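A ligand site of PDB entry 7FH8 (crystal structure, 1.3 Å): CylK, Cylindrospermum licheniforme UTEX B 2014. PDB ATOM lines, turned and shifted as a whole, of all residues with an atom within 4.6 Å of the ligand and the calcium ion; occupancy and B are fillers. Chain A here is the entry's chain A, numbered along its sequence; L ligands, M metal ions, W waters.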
ATOM      1  N   TYR A  37      -9.139  34.874   0.102  1.00  0.00           N
ATOM      2  CA  TYR A  37      -9.979  33.691   0.238  1.00  0.00           C
ATOM      3  C   TYR A  37      -9.593  32.875   1.473  1.00  0.00           C
ATOM      4  O   TYR A  37     -10.462  32.483   2.254  1.00  0.00           O
ATOM      5  CB  TYR A  37      -9.855  32.844  -1.033  1.00  0.00           C
ATOM      6  CG  TYR A  37     -10.867  31.738  -1.152  1.00  0.00           C
ATOM      7  CD1 TYR A  37     -12.216  32.021  -1.328  1.00  0.00           C
ATOM      8  CD2 TYR A  37     -10.471  30.409  -1.074  1.00  0.00           C
ATOM      9  CE1 TYR A  37     -13.151  31.007  -1.424  1.00  0.00           C
ATOM     10  CE2 TYR A  37     -11.404  29.388  -1.176  1.00  0.00           C
ATOM     11  CZ  TYR A  37     -12.730  29.697  -1.344  1.00  0.00           C
ATOM     12  OH  TYR A  37     -13.653  28.680  -1.448  1.00  0.00           O
ATOM     13  N   ILE A  38      -8.297  32.622   1.663  1.00  0.00           N
ATOM     14  CA  ILE A  38      -7.837  31.777   2.772  1.00  0.00           C
ATOM     15  C   ILE A  38      -8.179  32.412   4.109  1.00  0.00           C
ATOM     16  O   ILE A  38      -8.663  31.740   5.034  1.00  0.00           O
ATOM     17  CB  ILE A  38      -6.326  31.523   2.666  1.00  0.00           C
ATOM     18  CG1 ILE A  38      -5.984  30.658   1.458  1.00  0.00           C
ATOM     19  CG2 ILE A  38      -5.813  30.843   3.934  1.00  0.00           C
ATOM     20  CD1 ILE A  38      -4.520  30.723   1.110  1.00  0.00           C
ATOM     21  N   VAL A  41     -11.708  31.813   5.019  1.00  0.00           N
ATOM     22  CA  VAL A  41     -12.056  30.431   5.340  1.00  0.00           C
ATOM     23  C   VAL A  41     -11.552  30.051   6.735  1.00  0.00           C
ATOM     24  O   VAL A  41     -12.300  29.479   7.536  1.00  0.00           O
ATOM     25  CB  VAL A  41     -11.523  29.482   4.255  1.00  0.00           C
ATOM     26  CG1 VAL A  41     -11.859  28.059   4.605  1.00  0.00           C
ATOM     27  CG2 VAL A  41     -12.114  29.856   2.904  1.00  0.00           C
ATOM     28  N   LEU A  42     -10.282  30.344   7.033  1.00  0.00           N
ATOM     29  CA  LEU A  42      -9.720  29.928   8.320  1.00  0.00           C
ATOM     30  C   LEU A  42     -10.452  30.574   9.494  1.00  0.00           C
ATOM     31  O   LEU A  42     -10.644  29.952  10.545  1.00  0.00           O
ATOM     32  CB  LEU A  42      -8.218  30.212   8.390  1.00  0.00           C
ATOM     33  CG  LEU A  42      -7.301  29.479   7.411  1.00  0.00           C
ATOM     34  CD1 LEU A  42      -5.863  29.958   7.560  1.00  0.00           C
ATOM     35  CD2 LEU A  42      -7.393  27.974   7.608  1.00  0.00           C
ATOM     36  N   PHE A  72      -9.972  32.555 -10.698  1.00  0.00           N
ATOM     37  CA  PHE A  72      -9.643  32.058  -9.366  1.00  0.00           C
ATOM     38  C   PHE A  72      -9.458  30.545  -9.289  1.00  0.00           C
ATOM     39  O   PHE A  72      -8.570  30.083  -8.546  1.00  0.00           O
ATOM     40  CB  PHE A  72     -10.593  32.555  -8.273  1.00  0.00           C
ATOM     41  CG  PHE A  72     -10.093  32.257  -6.889  1.00  0.00           C
ATOM     42  CD1 PHE A  72      -8.958  32.892  -6.402  1.00  0.00           C
ATOM     43  CD2 PHE A  72     -10.745  31.350  -6.077  1.00  0.00           C
ATOM     44  CE1 PHE A  72      -8.473  32.604  -5.131  1.00  0.00           C
ATOM     45  CE2 PHE A  72     -10.283  31.062  -4.809  1.00  0.00           C
ATOM     46  CZ  PHE A  72      -9.146  31.689  -4.330  1.00  0.00           C
ATOM     47  N   PRO A  73     -10.252  29.723  -9.989  1.00  0.00           N
ATOM     48  CA  PRO A  73      -9.925  28.291 -10.022  1.00  0.00           C
ATOM     49  C   PRO A  73      -8.482  28.028 -10.432  1.00  0.00           C
ATOM     50  O   PRO A  73      -7.826  27.190  -9.804  1.00  0.00           O
ATOM     51  CB  PRO A  73     -10.969  27.714 -10.974  1.00  0.00           C
ATOM     52  CG  PRO A  73     -12.180  28.577 -10.700  1.00  0.00           C
ATOM     53  CD  PRO A  73     -11.584  29.972 -10.583  1.00  0.00           C
ATOM     54  N   PHE A  76      -6.262  29.150  -7.339  1.00  0.00           N
ATOM     55  CA  PHE A  76      -6.363  28.190  -6.247  1.00  0.00           C
ATOM     56  C   PHE A  76      -5.616  26.902  -6.578  1.00  0.00           C
ATOM     57  O   PHE A  76      -4.871  26.373  -5.755  1.00  0.00           O
ATOM     58  CB  PHE A  76      -7.826  27.904  -5.907  1.00  0.00           C
ATOM     59  CG  PHE A  76      -7.982  27.172  -4.625  1.00  0.00           C
ATOM     60  CD1 PHE A  76      -8.058  27.863  -3.432  1.00  0.00           C
ATOM     61  CD2 PHE A  76      -7.983  25.789  -4.603  1.00  0.00           C
ATOM     62  CE1 PHE A  76      -8.179  27.192  -2.232  1.00  0.00           C
ATOM     63  CE2 PHE A  76      -8.089  25.109  -3.405  1.00  0.00           C
ATOM     64  CZ  PHE A  76      -8.183  25.816  -2.217  1.00  0.00           C
ATOM     65  N   VAL A  82      -5.657  19.637  -3.871  1.00  0.00           N
ATOM     66  CA  VAL A  82      -6.957  19.277  -3.310  1.00  0.00           C
ATOM     67  C   VAL A  82      -7.160  17.792  -3.569  1.00  0.00           C
ATOM     68  O   VAL A  82      -7.255  17.351  -4.719  1.00  0.00           O
ATOM     69  CB  VAL A  82      -8.093  20.103  -3.939  1.00  0.00           C
ATOM     70  CG1 VAL A  82      -9.411  19.667  -3.348  1.00  0.00           C
ATOM     71  CG2 VAL A  82      -7.870  21.588  -3.690  1.00  0.00           C
ATOM     72  N   TRP A 103      -4.665  19.516   0.962  1.00  0.00           N
ATOM     73  CA  TRP A 103      -5.964  19.416   1.621  1.00  0.00           C
ATOM     74  C   TRP A 103      -6.491  17.988   1.451  1.00  0.00           C
ATOM     75  O   TRP A 103      -6.921  17.594   0.372  1.00  0.00           O
ATOM     76  CB  TRP A 103      -6.913  20.447   1.026  1.00  0.00           C
ATOM     77  CG  TRP A 103      -8.257  20.527   1.667  1.00  0.00           C
ATOM     78  CD1 TRP A 103      -8.607  20.091   2.915  1.00  0.00           C
ATOM     79  CD2 TRP A 103      -9.442  21.073   1.094  1.00  0.00           C
ATOM     80  NE1 TRP A 103      -9.939  20.348   3.154  1.00  0.00           N
ATOM     81  CE2 TRP A 103     -10.467  20.959   2.051  1.00  0.00           C
ATOM     82  CE3 TRP A 103      -9.736  21.659  -0.150  1.00  0.00           C
ATOM     83  CZ2 TRP A 103     -11.769  21.385   1.800  1.00  0.00           C
ATOM     84  CZ3 TRP A 103     -11.030  22.073  -0.387  1.00  0.00           C
ATOM     85  CH2 TRP A 103     -12.033  21.938   0.582  1.00  0.00           C
ATOM     86  N   ARG A 105      -9.166  16.427   2.898  1.00  0.00           N
ATOM     87  CA  ARG A 105     -10.621  16.215   2.937  1.00  0.00           C
ATOM     88  C   ARG A 105     -10.940  14.903   3.651  1.00  0.00           C
ATOM     89  O   ARG A 105     -10.172  14.444   4.509  1.00  0.00           O
ATOM     90  CB  ARG A 105     -11.267  16.422   1.570  1.00  0.00           C
ATOM     91  CG  ARG A 105     -11.118  17.854   1.073  1.00  0.00           C
ATOM     92  CD  ARG A 105     -11.508  18.006  -0.386  1.00  0.00           C
ATOM     93  NE  ARG A 105     -12.917  17.770  -0.655  1.00  0.00           N
ATOM     94  CZ  ARG A 105     -13.390  17.098  -1.695  1.00  0.00           C
ATOM     95  NH1 ARG A 105     -12.576  16.529  -2.573  1.00  0.00           N
ATOM     96  NH2 ARG A 105     -14.713  17.018  -1.875  1.00  0.00           N
ATOM     97  N   LEU A 130      -3.838  20.392   5.639  1.00  0.00           N
ATOM     98  CA  LEU A 130      -5.139  20.207   6.282  1.00  0.00           C
ATOM     99  C   LEU A 130      -5.486  18.730   6.141  1.00  0.00           C
ATOM    100  O   LEU A 130      -5.786  18.251   5.044  1.00  0.00           O
ATOM    101  CB  LEU A 130      -6.204  21.084   5.616  1.00  0.00           C
ATOM    102  CG  LEU A 130      -6.011  22.597   5.775  1.00  0.00           C
ATOM    103  CD1 LEU A 130      -6.735  23.328   4.655  1.00  0.00           C
ATOM    104  CD2 LEU A 130      -6.556  23.035   7.124  1.00  0.00           C
ATOM    105  N   PHE A 133     -10.538  18.980   7.489  1.00  0.00           N
ATOM    106  CA  PHE A 133     -11.166  20.232   7.082  1.00  0.00           C
ATOM    107  C   PHE A 133     -12.235  19.958   6.022  1.00  0.00           C
ATOM    108  O   PHE A 133     -12.187  20.500   4.907  1.00  0.00           O
ATOM    109  CB  PHE A 133     -10.076  21.185   6.572  1.00  0.00           C
ATOM    110  CG  PHE A 133     -10.358  22.649   6.781  1.00  0.00           C
ATOM    111  CD1 PHE A 133     -10.219  23.221   8.037  1.00  0.00           C
ATOM    112  CD2 PHE A 133     -10.726  23.448   5.710  1.00  0.00           C
ATOM    113  CE1 PHE A 133     -10.459  24.572   8.225  1.00  0.00           C
ATOM    114  CE2 PHE A 133     -10.967  24.799   5.897  1.00  0.00           C
ATOM    115  CZ  PHE A 133     -10.834  25.361   7.148  1.00  0.00           C
ATOM    116  N   ASP A 135     -15.658  19.210   3.664  1.00  0.00           N
ATOM    117  CA  ASP A 135     -16.614  20.086   2.994  1.00  0.00           C
ATOM    118  C   ASP A 135     -17.767  20.456   3.914  1.00  0.00           C
ATOM    119  O   ASP A 135     -18.262  21.598   3.887  1.00  0.00           O
ATOM    120  CB  ASP A 135     -17.194  19.372   1.774  1.00  0.00           C
ATOM    121  CG  ASP A 135     -16.133  18.851   0.800  1.00  0.00           C
ATOM    122  OD1 ASP A 135     -14.933  18.772   1.140  1.00  0.00           O
ATOM    123  OD2 ASP A 135     -16.526  18.480  -0.324  1.00  0.00           O
ATOM    124  N   PHE A 138     -16.395  23.112   5.916  1.00  0.00           N
ATOM    125  CA  PHE A 138     -16.263  24.244   5.001  1.00  0.00           C
ATOM    126  C   PHE A 138     -17.610  24.873   4.667  1.00  0.00           C
ATOM    127  O   PHE A 138     -17.726  26.102   4.574  1.00  0.00           O
ATOM    128  CB  PHE A 138     -15.527  23.814   3.741  1.00  0.00           C
ATOM    129  CG  PHE A 138     -15.550  24.830   2.638  1.00  0.00           C
ATOM    130  CD1 PHE A 138     -14.600  25.829   2.566  1.00  0.00           C
ATOM    131  CD2 PHE A 138     -16.514  24.759   1.640  1.00  0.00           C
ATOM    132  CE1 PHE A 138     -14.649  26.765   1.552  1.00  0.00           C
ATOM    133  CE2 PHE A 138     -16.548  25.679   0.617  1.00  0.00           C
ATOM    134  CZ  PHE A 138     -15.614  26.678   0.569  1.00  0.00           C
ATOM    135  N   ASN A 139     -18.643  24.057   4.483  1.00  0.00           N
ATOM    136  CA  ASN A 139     -19.954  24.549   4.050  1.00  0.00           C
ATOM    137  C   ASN A 139     -21.042  23.718   4.710  1.00  0.00           C
ATOM    138  O   ASN A 139     -21.506  22.724   4.150  1.00  0.00           O
ATOM    139  CB  ASN A 139     -20.082  24.511   2.521  1.00  0.00           C
ATOM    140  CG  ASN A 139     -21.419  25.016   2.041  1.00  0.00           C
ATOM    141  OD1 ASN A 139     -22.028  25.892   2.654  1.00  0.00           O
ATOM    142  ND2 ASN A 139     -21.884  24.470   0.920  1.00  0.00           N
ATOM    143  N   GLU A 374      -8.803  18.737 -15.950  1.00  0.00           N
ATOM    144  CA  GLU A 374      -8.107  17.551 -15.509  1.00  0.00           C
ATOM    145  C   GLU A 374      -8.569  16.393 -16.390  1.00  0.00           C
ATOM    146  O   GLU A 374      -9.654  16.444 -16.979  1.00  0.00           O
ATOM    147  CB  GLU A 374      -8.341  17.244 -14.024  1.00  0.00           C
ATOM    148  CG  GLU A 374      -9.793  17.114 -13.638  1.00  0.00           C
ATOM    149  CD  GLU A 374      -9.972  16.860 -12.152  1.00  0.00           C
ATOM    150  OE1 GLU A 374      -9.139  17.360 -11.366  1.00  0.00           O
ATOM    151  OE2 GLU A 374     -10.945  16.177 -11.772  1.00  0.00           O
ATOM    152  N   PHE A 393     -13.531  23.275 -15.625  1.00  0.00           N
ATOM    153  CA  PHE A 393     -14.209  24.444 -15.090  1.00  0.00           C
ATOM    154  C   PHE A 393     -14.677  25.394 -16.190  1.00  0.00           C
ATOM    155  O   PHE A 393     -15.300  26.420 -15.885  1.00  0.00           O
ATOM    156  CB  PHE A 393     -13.274  25.222 -14.160  1.00  0.00           C
ATOM    157  CG  PHE A 393     -13.136  24.617 -12.801  1.00  0.00           C
ATOM    158  CD1 PHE A 393     -12.205  23.612 -12.564  1.00  0.00           C
ATOM    159  CD2 PHE A 393     -13.904  25.081 -11.738  1.00  0.00           C
ATOM    160  CE1 PHE A 393     -12.056  23.066 -11.304  1.00  0.00           C
ATOM    161  CE2 PHE A 393     -13.757  24.541 -10.471  1.00  0.00           C
ATOM    162  CZ  PHE A 393     -12.835  23.525 -10.253  1.00  0.00           C
ATOM    163  N   GLN A 401     -22.227  24.302 -17.144  1.00  0.00           N
ATOM    164  CA  GLN A 401     -23.526  24.415 -16.484  1.00  0.00           C
ATOM    165  C   GLN A 401     -23.541  25.584 -15.497  1.00  0.00           C
ATOM    166  O   GLN A 401     -24.618  26.128 -15.205  1.00  0.00           O
ATOM    167  CB  GLN A 401     -23.872  23.130 -15.745  1.00  0.00           C
ATOM    168  CG  GLN A 401     -24.046  21.891 -16.615  1.00  0.00           C
ATOM    169  CD  GLN A 401     -25.238  21.978 -17.547  1.00  0.00           C
ATOM    170  OE1 GLN A 401     -26.300  22.451 -17.167  1.00  0.00           O
ATOM    171  NE2 GLN A 401     -25.048  21.524 -18.782  1.00  0.00           N
ATOM    172  N   GLU A 410     -22.894  30.412  -6.735  1.00  0.00           N
ATOM    173  CA  GLU A 410     -22.617  28.991  -6.831  1.00  0.00           C
ATOM    174  C   GLU A 410     -21.133  28.866  -7.142  1.00  0.00           C
ATOM    175  O   GLU A 410     -20.674  29.360  -8.168  1.00  0.00           O
ATOM    176  CB  GLU A 410     -23.459  28.337  -7.922  1.00  0.00           C
ATOM    177  CG  GLU A 410     -23.202  26.840  -8.104  1.00  0.00           C
ATOM    178  CD  GLU A 410     -23.793  26.023  -6.970  1.00  0.00           C
ATOM    179  OE1 GLU A 410     -24.942  26.315  -6.571  1.00  0.00           O
ATOM    180  OE2 GLU A 410     -23.134  25.074  -6.502  1.00  0.00           O
ATOM    181  N   LEU A 411     -20.399  28.210  -6.252  1.00  0.00           N
ATOM    182  CA  LEU A 411     -18.957  28.112  -6.385  1.00  0.00           C
ATOM    183  C   LEU A 411     -18.595  27.569  -7.767  1.00  0.00           C
ATOM    184  O   LEU A 411     -19.239  26.624  -8.241  1.00  0.00           O
ATOM    185  CB  LEU A 411     -18.434  27.147  -5.316  1.00  0.00           C
ATOM    186  CG  LEU A 411     -16.928  27.049  -5.078  1.00  0.00           C
ATOM    187  CD1 LEU A 411     -16.398  28.297  -4.387  1.00  0.00           C
ATOM    188  CD2 LEU A 411     -16.614  25.802  -4.257  1.00  0.00           C
ATOM    189  N   PRO A 412     -17.590  28.138  -8.440  1.00  0.00           N
ATOM    190  CA  PRO A 412     -17.152  27.587  -9.727  1.00  0.00           C
ATOM    191  C   PRO A 412     -16.973  26.079  -9.613  1.00  0.00           C
ATOM    192  O   PRO A 412     -16.482  25.567  -8.603  1.00  0.00           O
ATOM    193  CB  PRO A 412     -15.799  28.271  -9.972  1.00  0.00           C
ATOM    194  CG  PRO A 412     -15.842  29.507  -9.200  1.00  0.00           C
ATOM    195  CD  PRO A 412     -16.774  29.299  -8.030  1.00  0.00           C
ATOM    196  N   SER A 413     -17.383  25.379 -10.670  1.00  0.00           N
ATOM    197  CA  SER A 413     -17.486  23.923 -10.596  1.00  0.00           C
ATOM    198  C   SER A 413     -17.214  23.290 -11.949  1.00  0.00           C
ATOM    199  O   SER A 413     -17.351  23.908 -13.007  1.00  0.00           O
ATOM    200  CB  SER A 413     -18.873  23.513 -10.074  1.00  0.00           C
ATOM    201  OG  SER A 413     -19.884  24.162 -10.829  1.00  0.00           O
ATOM    202  N   THR A 414     -16.847  22.019 -11.891  1.00  0.00           N
ATOM    203  CA  THR A 414     -16.548  21.258 -13.097  1.00  0.00           C
ATOM    204  C   THR A 414     -17.788  20.629 -13.710  1.00  0.00           C
ATOM    205  O   THR A 414     -18.764  20.316 -13.029  1.00  0.00           O
ATOM    206  CB  THR A 414     -15.558  20.140 -12.806  1.00  0.00           C
ATOM    207  OG1 THR A 414     -16.031  19.372 -11.696  1.00  0.00           O
ATOM    208  CG2 THR A 414     -14.208  20.734 -12.534  1.00  0.00           C
ATOM    209  N   ASP A 415     -17.697  20.410 -15.014  1.00  0.00           N
ATOM    210  CA  ASP A 415     -18.537  19.486 -15.765  1.00  0.00           C
ATOM    211  C   ASP A 415     -17.639  18.360 -16.270  1.00  0.00           C
ATOM    212  O   ASP A 415     -16.418  18.515 -16.386  1.00  0.00           O
ATOM    213  CB  ASP A 415     -19.148  20.187 -16.989  1.00  0.00           C
ATOM    214  CG  ASP A 415     -20.244  21.165 -16.620  1.00  0.00           C
ATOM    215  OD1 ASP A 415     -20.762  21.142 -15.477  1.00  0.00           O
ATOM    216  OD2 ASP A 415     -20.608  21.957 -17.527  1.00  0.00           O
ATOM    217  N   THR A 435     -24.182  19.002 -14.108  1.00  0.00           N
ATOM    218  CA  THR A 435     -25.100  19.812 -13.306  1.00  0.00           C
ATOM    219  C   THR A 435     -24.416  21.134 -12.956  1.00  0.00           C
ATOM    220  O   THR A 435     -23.243  21.340 -13.262  1.00  0.00           O
ATOM    221  CB  THR A 435     -25.449  19.116 -11.985  1.00  0.00           C
ATOM    222  OG1 THR A 435     -24.290  19.054 -11.157  1.00  0.00           O
ATOM    223  CG2 THR A 435     -25.976  17.704 -12.229  1.00  0.00           C
ATOM    224  N   ILE A 436     -25.157  22.017 -12.277  1.00  0.00           N
ATOM    225  CA  ILE A 436     -24.572  23.291 -11.855  1.00  0.00           C
ATOM    226  C   ILE A 436     -23.445  23.107 -10.841  1.00  0.00           C
ATOM    227  O   ILE A 436     -22.627  24.019 -10.654  1.00  0.00           O
ATOM    228  CB  ILE A 436     -25.664  24.238 -11.313  1.00  0.00           C
ATOM    229  CG1 ILE A 436     -25.186  25.686 -11.344  1.00  0.00           C
ATOM    230  CG2 ILE A 436     -26.060  23.827  -9.915  1.00  0.00           C
ATOM    231  CD1 ILE A 436     -26.257  26.689 -10.966  1.00  0.00           C
ATOM    232  N   THR A 437     -23.380  21.967 -10.162  1.00  0.00           N
ATOM    233  CA  THR A 437     -22.381  21.754  -9.130  1.00  0.00           C
ATOM    234  C   THR A 437     -21.253  20.859  -9.661  1.00  0.00           C
ATOM    235  O   THR A 437     -21.073  20.730 -10.879  1.00  0.00           O
ATOM    236  CB  THR A 437     -23.064  21.296  -7.831  1.00  0.00           C
ATOM    237  OG1 THR A 437     -22.088  21.180  -6.772  1.00  0.00           O
ATOM    238  CG2 THR A 437     -23.787  19.957  -8.029  1.00  0.00           C
ATOM    239  N   LEU A 438     -20.476  20.267  -8.754  1.00  0.00           N
ATOM    240  CA  LEU A 438     -19.353  19.414  -9.114  1.00  0.00           C
ATOM    241  C   LEU A 438     -19.811  18.173  -9.869  1.00  0.00           C
ATOM    242  O   LEU A 438     -20.651  17.406  -9.378  1.00  0.00           O
ATOM    243  CB  LEU A 438     -18.610  19.011  -7.831  1.00  0.00           C
ATOM    244  CG  LEU A 438     -17.371  18.096  -7.905  1.00  0.00           C
ATOM    245  CD1 LEU A 438     -16.586  18.283  -6.631  1.00  0.00           C
ATOM    246  CD2 LEU A 438     -17.730  16.615  -8.058  1.00  0.00           C
ATOM    247  N   ASP A 439     -19.240  17.966 -11.057  1.00  0.00           N
ATOM    248  CA  ASP A 439     -19.308  16.684 -11.763  1.00  0.00           C
ATOM    249  C   ASP A 439     -17.899  16.401 -12.274  1.00  0.00           C
ATOM    250  O   ASP A 439     -17.355  17.179 -13.066  1.00  0.00           O
ATOM    251  CB  ASP A 439     -20.272  16.730 -12.963  1.00  0.00           C
ATOM    252  CG  ASP A 439     -21.489  17.575 -12.701  1.00  0.00           C
ATOM    253  OD1 ASP A 439     -22.404  17.142 -11.959  1.00  0.00           O
ATOM    254  OD2 ASP A 439     -21.573  18.669 -13.294  1.00  0.00           O
ATOM    255  N   ASP A 440     -17.297  15.313 -11.822  1.00  0.00           N
ATOM    256  CA  ASP A 440     -15.952  14.888 -12.176  1.00  0.00           C
ATOM    257  C   ASP A 440     -16.028  13.612 -13.018  1.00  0.00           C
ATOM    258  O   ASP A 440     -17.015  12.873 -12.927  1.00  0.00           O
ATOM    259  CB  ASP A 440     -15.153  14.560 -10.901  1.00  0.00           C
ATOM    260  CG  ASP A 440     -14.751  15.794 -10.107  1.00  0.00           C
ATOM    261  OD1 ASP A 440     -14.840  16.923 -10.651  1.00  0.00           O
ATOM    262  OD2 ASP A 440     -14.359  15.630  -8.935  1.00  0.00           O
ATOM    263  N   LYS A 459     -21.975  15.922  -7.131  1.00  0.00           N
ATOM    264  CA  LYS A 459     -22.671  16.407  -5.946  1.00  0.00           C
ATOM    265  C   LYS A 459     -24.128  16.746  -6.214  1.00  0.00           C
ATOM    266  O   LYS A 459     -24.855  17.076  -5.279  1.00  0.00           O
ATOM    267  CB  LYS A 459     -21.977  17.670  -5.392  1.00  0.00           C
ATOM    268  CG  LYS A 459     -20.615  17.402  -4.744  1.00  0.00           C
ATOM    269  CD  LYS A 459     -19.920  18.689  -4.242  1.00  0.00           C
ATOM    270  CE  LYS A 459     -20.737  19.492  -3.228  1.00  0.00           C
ATOM    271  NZ  LYS A 459     -21.122  18.691  -2.024  1.00  0.00           N
HETATM  272  C1  LIG L   1     -12.504  26.197  -4.386  1.00  0.00           C
HETATM  273  C2  LIG L   1     -12.211  25.705  -6.932  1.00  0.00           C
HETATM  274  C3  LIG L   1     -13.635  23.611  -6.794  1.00  0.00           C
HETATM  275  C4  LIG L   1     -12.483  18.994  -7.520  1.00  0.00           C
HETATM  276  C5  LIG L   1     -13.525  18.731  -8.529  1.00  0.00           C
HETATM  277  C6  LIG L   1     -13.188  19.422  -9.761  1.00  0.00           C
HETATM  278  C7  LIG L   1     -12.525  19.207  -5.059  1.00  0.00           C
HETATM  279  C8  LIG L   1     -14.218  20.343  -3.573  1.00  0.00           C
HETATM  280  C9  LIG L   1     -15.692  21.907  -2.254  1.00  0.00           C
HETATM  281  C10 LIG L   1      -7.808  27.063   3.537  1.00  0.00           C
HETATM  282  C11 LIG L   1      -8.610  25.846   3.086  1.00  0.00           C
HETATM  283  C12 LIG L   1      -9.448  26.096   1.837  1.00  0.00           C
HETATM  284  C13 LIG L   1     -10.528  25.039   1.640  1.00  0.00           C
HETATM  285  C14 LIG L   1     -11.630  25.514   0.682  1.00  0.00           C
HETATM  286  C15 LIG L   1     -11.175  25.377  -0.771  1.00  0.00           C
HETATM  287  C16 LIG L   1     -12.207  25.798  -1.817  1.00  0.00           C
HETATM  288  C17 LIG L   1     -11.553  25.871  -3.224  1.00  0.00           C
HETATM  289  C18 LIG L   1     -11.725  26.518  -5.702  1.00  0.00           C
HETATM  290  C19 LIG L   1     -11.870  27.989  -5.999  1.00  0.00           C
HETATM  291  C20 LIG L   1     -12.380  24.199  -6.793  1.00  0.00           C
HETATM  292  C21 LIG L   1     -13.814  22.231  -6.669  1.00  0.00           C
HETATM  293  C22 LIG L   1     -12.764  21.322  -6.531  1.00  0.00           C
HETATM  294  C23 LIG L   1     -13.044  19.801  -6.371  1.00  0.00           C
HETATM  295  C24 LIG L   1     -11.931  18.863 -10.386  1.00  0.00           C
HETATM  296  C25 LIG L   1     -12.746  20.099  -3.853  1.00  0.00           C
HETATM  297  C26 LIG L   1     -14.449  21.047  -2.253  1.00  0.00           C
HETATM  298  C27 LIG L   1     -15.801  22.653  -0.951  1.00  0.00           C
HETATM  299  C28 LIG L   1     -16.998  21.101  -2.462  1.00  0.00           C
HETATM  300  C29 LIG L   1     -18.083  21.864  -3.132  1.00  0.00           C
HETATM  301  C30 LIG L   1     -19.007  22.588  -2.375  1.00  0.00           C
HETATM  302  C31 LIG L   1     -20.012  23.314  -2.992  1.00  0.00           C
HETATM  303  C32 LIG L   1     -20.139  23.373  -4.376  1.00  0.00           C
HETATM  304  C33 LIG L   1     -19.195  22.658  -5.123  1.00  0.00           C
HETATM  305  C34 LIG L   1     -18.174  21.915  -4.515  1.00  0.00           C
HETATM  306  C35 LIG L   1     -11.484  21.928  -6.528  1.00  0.00           C
HETATM  307  C36 LIG L   1     -11.287  23.315  -6.657  1.00  0.00           C
HETATM  308  F1  LIG L   1     -11.860  26.831   0.963  1.00  0.00           F
HETATM  309  O1  LIG L   1     -15.100  21.768  -6.687  1.00  0.00           O
HETATM  310  O2  LIG L   1     -20.886  23.973  -2.174  1.00  0.00           O
HETATM  311  O3  LIG L   1     -19.238  22.660  -6.475  1.00  0.00           O
HETATM  312  O4  LIG L   1     -10.420  21.085  -6.396  1.00  0.00           O
HETATM  313 CA    CA M   1     -21.019  20.879 -13.200  1.00  0.00          CA
HETATM  314  O   HOH W   1      -9.219  24.854  -8.434  1.00  0.00           O
HETATM  315  O   HOH W   2     -20.729  24.459  -7.491  1.00  0.00           O
HETATM  316  O   HOH W   3      -8.160  22.367  -7.464  1.00  0.00           O
HETATM  317  O   HOH W   4     -20.409  23.153 -13.299  1.00  0.00           O
HETATM  318  O   HOH W   5     -16.212  21.101  -9.190  1.00  0.00           O
HETATM  319  O   HOH W   6     -21.626  26.931  -3.704  1.00  0.00           O
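The side-chain hydroxyl of Thr 437 lies within hydrogen-bond range of an oxygen (O3) of the ligand, 3.2 Å away. The side-chain amide nitrogen (ND2) of Asn 139 is in hydrogen-bond range of an oxygen (O2) of the ligand, at 3.3 Å.
OG1 of Thr 435 sits close to N of Thr 437 (3.2 Å). N of Gln 401 lies within hydrogen-bond range of OD2 of Asp 415, 2.9 Å away. OD1 of Asp 440 lies within hydrogen-bond range of OG1 of Thr 414 (2.9 Å). O of Phe 133 lies within hydrogen-bond range of NE1 of Trp 103, at 2.9 Å. The side-chain carboxylate (OD2) of Asp 135 lies within salt-bridge range of the guanidinium group (NH2) of Arg 105, at 2.8 Å. The backbone carbonyl oxygen (O) of Leu 438 is in hydrogen-bond range of the backbone NH (N) of Lys 459, 3.0 Å away. The backbone carbonyl oxygen of Ile 436 sits at hydrogen-bond distance from the side-chain hydroxyl of Ser 413 (2.8 Å).
Tyr 37 touches the ligand. Val 41 touches the ligand (CG2 to F1, 3.6 Å). Phe 72 touches the ligand. Phe 76 touches the ligand. CG1 of Val 82 touches C25 of the ligand, 3.4 Å away. Trp 103 touches the ligand. Arg 105 touches the ligand (NH1 to C7, 3.7 Å). Leu 130 touches the ligand (CD1 to C11, 3.5 Å). Phe 133 touches the ligand (CE2 to C11, 3.8 Å). Asp 135 touches the ligand (OD2 to C28, 3.4 Å). CE1 of Phe 138 touches F1 of the ligand, 2.9 Å away. Glu 374 touches the ligand. CZ of Phe 393 touches C3 of the ligand (3.6 Å). Pro 412 touches the ligand (O to C3, 3.9 Å). Ser 413 touches the ligand (CB to O3, 3.7 Å). N of Leu 438 touches O3 of the ligand (3.5 Å). OD1 of Asp 440 touches C5 of the ligand (3.1 Å). Lys 459 touches the ligand (CE to C29, 3.6 Å). 21 residues have an atom within 4 Å of the ligand: Tyr 37, Val 41, Phe 72, Phe 76, Val 82, Trp 103, Arg 105, Leu 130, Phe 133, Asp 135, Phe 138, Asn 139, Glu 374, Phe 393, Pro 412, Ser 413, Thr 414, Thr 437, Leu 438, Asp 440 and Lys 459.
Of the 31 residues printed, 5 come within 4 Å of the calcium ion.
O of Thr 435 is bound to the calcium ion, 2.3 Å away. OD2 of Asp 439 is bound to the calcium ion. OD1 of Asp 415 binds the calcium ion (2.3 Å). The calcium ion is bound by the backbone carbonyl oxygen (O) of Thr 437, at 2.3 Å. O of Thr 414 is bound to the calcium ion, at 2.3 Å. The calcium ion is bound by water W4 (2.4 Å). The calcium ion has six donor atoms within binding distance.
Water W2 lies within hydrogen-bond range of O3 of the ligand (2.5 Å), OE2 of Glu 410 (2.7 Å), O of Leu 411 (2.7 Å) and OG of Ser 413 (3.5 Å). Water W5 lies within hydrogen-bond range of an oxygen (O1) of the ligand (2.8 Å) and the backbone NH of Thr 414 (2.9 Å). Water W6 bridges the backbone NH (N) of Leu 411 (3.1 Å) and an oxygen (O2) of the ligand (3.4 Å).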
